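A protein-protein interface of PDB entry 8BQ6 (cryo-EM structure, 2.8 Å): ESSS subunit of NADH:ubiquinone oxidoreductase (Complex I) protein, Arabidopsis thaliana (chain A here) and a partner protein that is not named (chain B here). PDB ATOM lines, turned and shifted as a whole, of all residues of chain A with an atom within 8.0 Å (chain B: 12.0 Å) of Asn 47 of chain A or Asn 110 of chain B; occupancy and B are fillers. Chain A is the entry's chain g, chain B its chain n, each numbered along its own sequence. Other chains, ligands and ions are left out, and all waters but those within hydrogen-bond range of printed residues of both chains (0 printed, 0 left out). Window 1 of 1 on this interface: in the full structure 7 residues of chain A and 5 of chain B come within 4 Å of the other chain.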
ATOM      1  N   LYS A  42      16.138 -16.126 -14.192  1.00  0.00           N
ATOM      2  CA  LYS A  42      17.346 -16.000 -13.392  1.00  0.00           C
ATOM      3  C   LYS A  42      17.997 -17.363 -13.190  1.00  0.00           C
ATOM      4  O   LYS A  42      17.323 -18.356 -12.902  1.00  0.00           O
ATOM      5  CB  LYS A  42      17.029 -15.344 -12.044  1.00  0.00           C
ATOM      6  CG  LYS A  42      15.813 -15.905 -11.325  1.00  0.00           C
ATOM      7  CD  LYS A  42      15.819 -15.539  -9.847  1.00  0.00           C
ATOM      8  CE  LYS A  42      15.292 -14.134  -9.586  1.00  0.00           C
ATOM      9  NZ  LYS A  42      13.813 -14.062  -9.728  1.00  0.00           N
ATOM     10  N   GLY A  43      19.316 -17.407 -13.369  1.00  0.00           N
ATOM     11  CA  GLY A  43      20.058 -18.644 -13.244  1.00  0.00           C
ATOM     12  C   GLY A  43      19.946 -19.516 -14.478  1.00  0.00           C
ATOM     13  O   GLY A  43      19.313 -19.177 -15.478  1.00  0.00           O
ATOM     14  N   TYR A  44      20.589 -20.676 -14.396  1.00  0.00           N
ATOM     15  CA  TYR A  44      20.563 -21.656 -15.469  1.00  0.00           C
ATOM     16  C   TYR A  44      20.189 -23.014 -14.906  1.00  0.00           C
ATOM     17  O   TYR A  44      20.613 -23.381 -13.806  1.00  0.00           O
ATOM     18  CB  TYR A  44      21.907 -21.733 -16.187  1.00  0.00           C
ATOM     19  CG  TYR A  44      22.154 -20.519 -17.032  1.00  0.00           C
ATOM     20  CD1 TYR A  44      21.205 -20.093 -17.947  1.00  0.00           C
ATOM     21  CD2 TYR A  44      23.313 -19.774 -16.891  1.00  0.00           C
ATOM     22  CE1 TYR A  44      21.409 -18.975 -18.709  1.00  0.00           C
ATOM     23  CE2 TYR A  44      23.527 -18.649 -17.650  1.00  0.00           C
ATOM     24  CZ  TYR A  44      22.571 -18.257 -18.561  1.00  0.00           C
ATOM     25  OH  TYR A  44      22.769 -17.136 -19.330  1.00  0.00           O
ATOM     26  N   PHE A  45      19.389 -23.748 -15.670  1.00  0.00           N
ATOM     27  CA  PHE A  45      18.901 -25.045 -15.232  1.00  0.00           C
ATOM     28  C   PHE A  45      20.050 -26.035 -15.108  1.00  0.00           C
ATOM     29  O   PHE A  45      20.718 -26.350 -16.097  1.00  0.00           O
ATOM     30  CB  PHE A  45      17.860 -25.555 -16.219  1.00  0.00           C
ATOM     31  CG  PHE A  45      17.250 -26.855 -15.827  1.00  0.00           C
ATOM     32  CD1 PHE A  45      16.672 -27.014 -14.584  1.00  0.00           C
ATOM     33  CD2 PHE A  45      17.267 -27.926 -16.697  1.00  0.00           C
ATOM     34  CE1 PHE A  45      16.115 -28.216 -14.221  1.00  0.00           C
ATOM     35  CE2 PHE A  45      16.705 -29.127 -16.341  1.00  0.00           C
ATOM     36  CZ  PHE A  45      16.133 -29.274 -15.100  1.00  0.00           C
ATOM     37  N   MET A  46      20.257 -26.538 -13.890  1.00  0.00           N
ATOM     38  CA  MET A  46      21.381 -27.413 -13.558  1.00  0.00           C
ATOM     39  C   MET A  46      22.719 -26.689 -13.692  1.00  0.00           C
ATOM     40  O   MET A  46      23.761 -27.325 -13.859  1.00  0.00           O
ATOM     41  CB  MET A  46      21.375 -28.695 -14.399  1.00  0.00           C
ATOM     42  CG  MET A  46      20.139 -29.557 -14.214  1.00  0.00           C
ATOM     43  SD  MET A  46      19.707 -30.514 -15.676  1.00  0.00           S
ATOM     44  CE  MET A  46      18.569 -31.696 -14.960  1.00  0.00           C
ATOM     45  N   ASN A  47      22.689 -25.355 -13.614  1.00  0.00           N
ATOM     46  CA  ASN A  47      23.890 -24.513 -13.568  1.00  0.00           C
ATOM     47  C   ASN A  47      24.846 -24.773 -14.725  1.00  0.00           C
ATOM     48  O   ASN A  47      26.066 -24.738 -14.550  1.00  0.00           O
ATOM     49  CB  ASN A  47      24.642 -24.670 -12.246  1.00  0.00           C
ATOM     50  CG  ASN A  47      23.964 -23.962 -11.103  1.00  0.00           C
ATOM     51  OD1 ASN A  47      22.746 -23.791 -11.097  1.00  0.00           O
ATOM     52  ND2 ASN A  47      24.753 -23.532 -10.128  1.00  0.00           N
ATOM     53  N   ARG A  48      24.320 -25.023 -15.914  1.00  0.00           N
ATOM     54  CA  ARG A  48      25.149 -25.164 -17.100  1.00  0.00           C
ATOM     55  C   ARG A  48      24.954 -23.940 -17.981  1.00  0.00           C
ATOM     56  O   ARG A  48      23.819 -23.584 -18.314  1.00  0.00           O
ATOM     57  CB  ARG A  48      24.813 -26.444 -17.862  1.00  0.00           C
ATOM     58  CG  ARG A  48      25.186 -27.715 -17.138  1.00  0.00           C
ATOM     59  CD  ARG A  48      24.662 -28.913 -17.890  1.00  0.00           C
ATOM     60  NE  ARG A  48      23.207 -28.931 -17.939  1.00  0.00           N
ATOM     61  CZ  ARG A  48      22.501 -29.878 -18.540  1.00  0.00           C
ATOM     62  NH1 ARG A  48      23.089 -30.901 -19.137  1.00  0.00           N
ATOM     63  NH2 ARG A  48      21.173 -29.800 -18.538  1.00  0.00           N
ATOM     64  N   THR A  49      26.058 -23.285 -18.328  1.00  0.00           N
ATOM     65  CA  THR A  49      25.988 -22.164 -19.247  1.00  0.00           C
ATOM     66  C   THR A  49      25.438 -22.643 -20.587  1.00  0.00           C
ATOM     67  O   THR A  49      25.781 -23.733 -21.051  1.00  0.00           O
ATOM     68  CB  THR A  49      27.365 -21.545 -19.450  1.00  0.00           C
ATOM     69  OG1 THR A  49      28.283 -22.559 -19.877  1.00  0.00           O
ATOM     70  CG2 THR A  49      27.872 -20.931 -18.156  1.00  0.00           C
ATOM     71  N   PRO A  50      24.568 -21.862 -21.218  1.00  0.00           N
ATOM     72  CA  PRO A  50      24.029 -22.259 -22.514  1.00  0.00           C
ATOM     73  C   PRO A  50      25.122 -22.304 -23.566  1.00  0.00           C
ATOM     74  O   PRO A  50      26.145 -21.615 -23.446  1.00  0.00           O
ATOM     75  CB  PRO A  50      23.000 -21.158 -22.808  1.00  0.00           C
ATOM     76  CG  PRO A  50      23.561 -19.973 -22.102  1.00  0.00           C
ATOM     77  CD  PRO A  50      24.007 -20.570 -20.790  1.00  0.00           C
ATOM     78  N   ILE B 105      28.900 -13.371  -2.069  1.00  0.00           N
ATOM     79  CA  ILE B 105      28.400 -14.681  -2.459  1.00  0.00           C
ATOM     80  C   ILE B 105      28.643 -14.844  -3.953  1.00  0.00           C
ATOM     81  O   ILE B 105      28.291 -13.962  -4.745  1.00  0.00           O
ATOM     82  CB  ILE B 105      26.907 -14.832  -2.130  1.00  0.00           C
ATOM     83  CG1 ILE B 105      26.629 -14.604  -0.638  1.00  0.00           C
ATOM     84  CG2 ILE B 105      26.411 -16.200  -2.548  1.00  0.00           C
ATOM     85  CD1 ILE B 105      27.516 -15.371   0.303  1.00  0.00           C
ATOM     86  N   GLU B 106      29.308 -15.943  -4.317  1.00  0.00           N
ATOM     87  CA  GLU B 106      29.581 -16.234  -5.744  1.00  0.00           C
ATOM     88  C   GLU B 106      28.922 -17.555  -6.131  1.00  0.00           C
ATOM     89  O   GLU B 106      28.873 -18.454  -5.286  1.00  0.00           O
ATOM     90  CB  GLU B 106      31.086 -16.296  -6.009  1.00  0.00           C
ATOM     91  CG  GLU B 106      31.806 -14.978  -5.801  1.00  0.00           C
ATOM     92  CD  GLU B 106      32.829 -15.021  -4.681  1.00  0.00           C
ATOM     93  OE1 GLU B 106      33.947 -14.509  -4.877  1.00  0.00           O
ATOM     94  OE2 GLU B 106      32.508 -15.578  -3.620  1.00  0.00           O
ATOM     95  N   ILE B 107      28.445 -17.663  -7.363  1.00  0.00           N
ATOM     96  CA  ILE B 107      27.761 -18.844  -7.875  1.00  0.00           C
ATOM     97  C   ILE B 107      28.596 -19.420  -9.007  1.00  0.00           C
ATOM     98  O   ILE B 107      28.902 -18.720  -9.980  1.00  0.00           O
ATOM     99  CB  ILE B 107      26.340 -18.506  -8.355  1.00  0.00           C
ATOM    100  CG1 ILE B 107      25.475 -18.017  -7.193  1.00  0.00           C
ATOM    101  CG2 ILE B 107      25.698 -19.713  -8.992  1.00  0.00           C
ATOM    102  CD1 ILE B 107      25.473 -18.930  -5.995  1.00  0.00           C
ATOM    103  N   VAL B 108      28.980 -20.688  -8.844  1.00  0.00           N
ATOM    104  CA  VAL B 108      29.844 -21.374  -9.843  1.00  0.00           C
ATOM    105  C   VAL B 108      28.992 -22.144 -10.849  1.00  0.00           C
ATOM    106  O   VAL B 108      28.098 -22.892 -10.418  1.00  0.00           O
ATOM    107  CB  VAL B 108      30.848 -22.309  -9.139  1.00  0.00           C
ATOM    108  CG1 VAL B 108      31.820 -22.966 -10.106  1.00  0.00           C
ATOM    109  CG2 VAL B 108      31.591 -21.607  -8.014  1.00  0.00           C
ATOM    110  N   TYR B 109      29.240 -21.943 -12.137  1.00  0.00           N
ATOM    111  CA  TYR B 109      28.576 -22.659 -13.214  1.00  0.00           C
ATOM    112  C   TYR B 109      29.486 -23.759 -13.738  1.00  0.00           C
ATOM    113  O   TYR B 109      30.713 -23.678 -13.626  1.00  0.00           O
ATOM    114  CB  TYR B 109      28.203 -21.719 -14.362  1.00  0.00           C
ATOM    115  CG  TYR B 109      27.085 -20.766 -14.033  1.00  0.00           C
ATOM    116  CD1 TYR B 109      26.134 -21.089 -13.080  1.00  0.00           C
ATOM    117  CD2 TYR B 109      26.973 -19.547 -14.683  1.00  0.00           C
ATOM    118  CE1 TYR B 109      25.110 -20.225 -12.777  1.00  0.00           C
ATOM    119  CE2 TYR B 109      25.947 -18.676 -14.388  1.00  0.00           C
ATOM    120  CZ  TYR B 109      25.019 -19.020 -13.434  1.00  0.00           C
ATOM    121  OH  TYR B 109      23.993 -18.157 -13.134  1.00  0.00           O
ATOM    122  N   ASN B 110      28.870 -24.786 -14.322  1.00  0.00           N
ATOM    123  CA  ASN B 110      29.594 -25.917 -14.909  1.00  0.00           C
ATOM    124  C   ASN B 110      30.518 -26.584 -13.890  1.00  0.00           C
ATOM    125  O   ASN B 110      31.710 -26.774 -14.135  1.00  0.00           O
ATOM    126  CB  ASN B 110      30.370 -25.488 -16.158  1.00  0.00           C
ATOM    127  CG  ASN B 110      29.575 -24.543 -17.042  1.00  0.00           C
ATOM    128  OD1 ASN B 110      28.520 -24.903 -17.561  1.00  0.00           O
ATOM    129  ND2 ASN B 110      30.075 -23.325 -17.211  1.00  0.00           N
ATOM    130  N   TYR B 111      29.958 -26.950 -12.740  1.00  0.00           N
ATOM    131  CA  TYR B 111      30.700 -27.688 -11.730  1.00  0.00           C
ATOM    132  C   TYR B 111      30.559 -29.190 -11.955  1.00  0.00           C
ATOM    133  O   TYR B 111      29.511 -29.678 -12.384  1.00  0.00           O
ATOM    134  CB  TYR B 111      30.204 -27.334 -10.325  1.00  0.00           C
ATOM    135  CG  TYR B 111      30.922 -28.094  -9.238  1.00  0.00           C
ATOM    136  CD1 TYR B 111      32.171 -27.691  -8.796  1.00  0.00           C
ATOM    137  CD2 TYR B 111      30.369 -29.239  -8.684  1.00  0.00           C
ATOM    138  CE1 TYR B 111      32.838 -28.389  -7.815  1.00  0.00           C
ATOM    139  CE2 TYR B 111      31.029 -29.946  -7.708  1.00  0.00           C
ATOM    140  CZ  TYR B 111      32.264 -29.517  -7.275  1.00  0.00           C
ATOM    141  OH  TYR B 111      32.925 -30.221  -6.298  1.00  0.00           O
ATOM    142  N   GLY B 112      31.630 -29.921 -11.654  1.00  0.00           N
ATOM    143  CA  GLY B 112      31.601 -31.374 -11.680  1.00  0.00           C
ATOM    144  C   GLY B 112      31.452 -32.010 -13.046  1.00  0.00           C
ATOM    145  O   GLY B 112      30.804 -33.054 -13.166  1.00  0.00           O
ATOM    146  N   LEU B 113      32.054 -31.422 -14.076  1.00  0.00           N
ATOM    147  CA  LEU B 113      31.993 -31.986 -15.416  1.00  0.00           C
ATOM    148  C   LEU B 113      32.927 -33.190 -15.532  1.00  0.00           C
ATOM    149  O   LEU B 113      33.912 -33.310 -14.799  1.00  0.00           O
ATOM    150  CB  LEU B 113      32.362 -30.918 -16.448  1.00  0.00           C
ATOM    151  CG  LEU B 113      31.577 -29.604 -16.371  1.00  0.00           C
ATOM    152  CD1 LEU B 113      31.944 -28.675 -17.511  1.00  0.00           C
ATOM    153  CD2 LEU B 113      30.083 -29.874 -16.384  1.00  0.00           C
ATOM    154  N   GLU B 114      32.609 -34.095 -16.465  1.00  0.00           N
ATOM    155  CA  GLU B 114      33.400 -35.317 -16.596  1.00  0.00           C
ATOM    156  C   GLU B 114      34.832 -35.028 -17.027  1.00  0.00           C
ATOM    157  O   GLU B 114      35.746 -35.781 -16.677  1.00  0.00           O
ATOM    158  CB  GLU B 114      32.748 -36.280 -17.585  1.00  0.00           C
ATOM    159  CG  GLU B 114      32.614 -35.733 -18.981  1.00  0.00           C
ATOM    160  CD  GLU B 114      32.242 -36.805 -19.971  1.00  0.00           C
ATOM    161  OE1 GLU B 114      31.601 -36.479 -20.987  1.00  0.00           O
ATOM    162  OE2 GLU B 114      32.603 -37.976 -19.738  1.00  0.00           O
ATOM    163  N   ASP B 115      35.046 -33.956 -17.779  1.00  0.00           N
ATOM    164  CA  ASP B 115      36.384 -33.577 -18.204  1.00  0.00           C
ATOM    165  C   ASP B 115      37.133 -32.863 -17.089  1.00  0.00           C
ATOM    166  O   ASP B 115      38.356 -32.742 -17.134  1.00  0.00           O
ATOM    167  CB  ASP B 115      36.310 -32.693 -19.446  1.00  0.00           C
ATOM    168  CG  ASP B 115      35.992 -33.481 -20.695  1.00  0.00           C
ATOM    169  OD1 ASP B 115      36.136 -34.720 -20.661  1.00  0.00           O
ATOM    170  OD2 ASP B 115      35.585 -32.866 -21.702  1.00  0.00           O
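O of Val 108 of chain B lies within hydrogen-bond range of ND2 of Asn 47 of chain A, 3.4 Å away.
O of Asn 47 of chain A lies within hydrogen-bond range of N of Asn 110 of chain B.
The side-chain amide oxygen of Asn 110 of chain B sits at hydrogen-bond distance from the backbone NH of Thr 49 of chain A (3.0 Å).
Of chain B, only Tyr 109 (3.97 Å) comes within 4 Å of Gly 43 of chain A.
Of the printed residues of chain B, Tyr 44 of chain A touches Tyr 109.
No residue of chain B comes within 4 Å of Phe 45 of chain A.
No residue of chain B comes within 4 Å of Met 46 of chain A.
Printed residues of chain B within 4 Å of Asn 47 of chain A: Val 108 (3.4 Å), Tyr 109 (3.5 Å) and Asn 110 (2.8 Å).
Arg 48 of chain A touches just one residue of chain B: Asn 110.
Thr 49 of chain A touches just these residues of chain B: Tyr 109 (3.8 Å) and Asn 110 (3.0 Å).
Printed residues of chain A within 4 Å of Val 108 of chain B: Asn 47 (3.4 Å).
Of the printed residues of chain A, Tyr 109 of chain B touches Gly 43 (3.97 Å), Tyr 44 (3.8 Å), Asn 47 (3.5 Å) and Thr 49 (3.8 Å).
Of chain A, only Asn 47, Arg 48 and Thr 49 come within 4 Å of Asn 110 of chain B.
The nearest residue of chain B that does not touch Asn 47 of chain A is Ile 107 of chain B (4.1 Å).
The nearest residue of chain A that does not touch Asn 110 of chain B is Met 46 of chain A (5.7 Å).
Tyr 109 of chain B touches Gly 43 of chain A (OH to CA, 3.97 Å).
Tyr 44 of chain A touches Tyr 109 of chain B (CD2 to CE2, 3.8 Å).
Tyr 109 of chain B touches Asn 47 of chain A (CA to O, 3.5 Å).
Asn 110 of chain B touches Arg 48 of chain A (OD1 to CA, 3.4 Å).
Thr 49 of chain A touches Tyr 109 of chain B (CG2 to CD2, 3.8 Å).
Of the 9 printed residues of chain A, 5 touch a printed residue of chain B.
Printed residues of chain A that touch a printed residue of chain B: Gly 43, Tyr 44, Asn 47, Arg 48 and Thr 49.
Hydrophobic or aromatic side chains of chain A within 4 Å of the printed part of chain B: Tyr 44.
Of the 11 printed residues of chain B, 3 touch a printed residue of chain A.
Printed residues of chain B that touch a printed residue of chain A: Val 108, Tyr 109 and Asn 110.
Along chain B the printed residues that touch a printed residue of chain A span positions 108 to 110.
Among the printed residues, no Asp or Glu carboxylate lies within 4 Å of a Lys or Arg side-chain nitrogen of the other chain.
O of Tyr 44 of chain A lies close to OD1 of Asn 47 of chain A.
The side-chain sulfur (SD) of Met 46 of chain A lies within hydrogen-bond range of the guanidinium group (NH2) of Arg 48 of chain A, 3.3 Å away.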
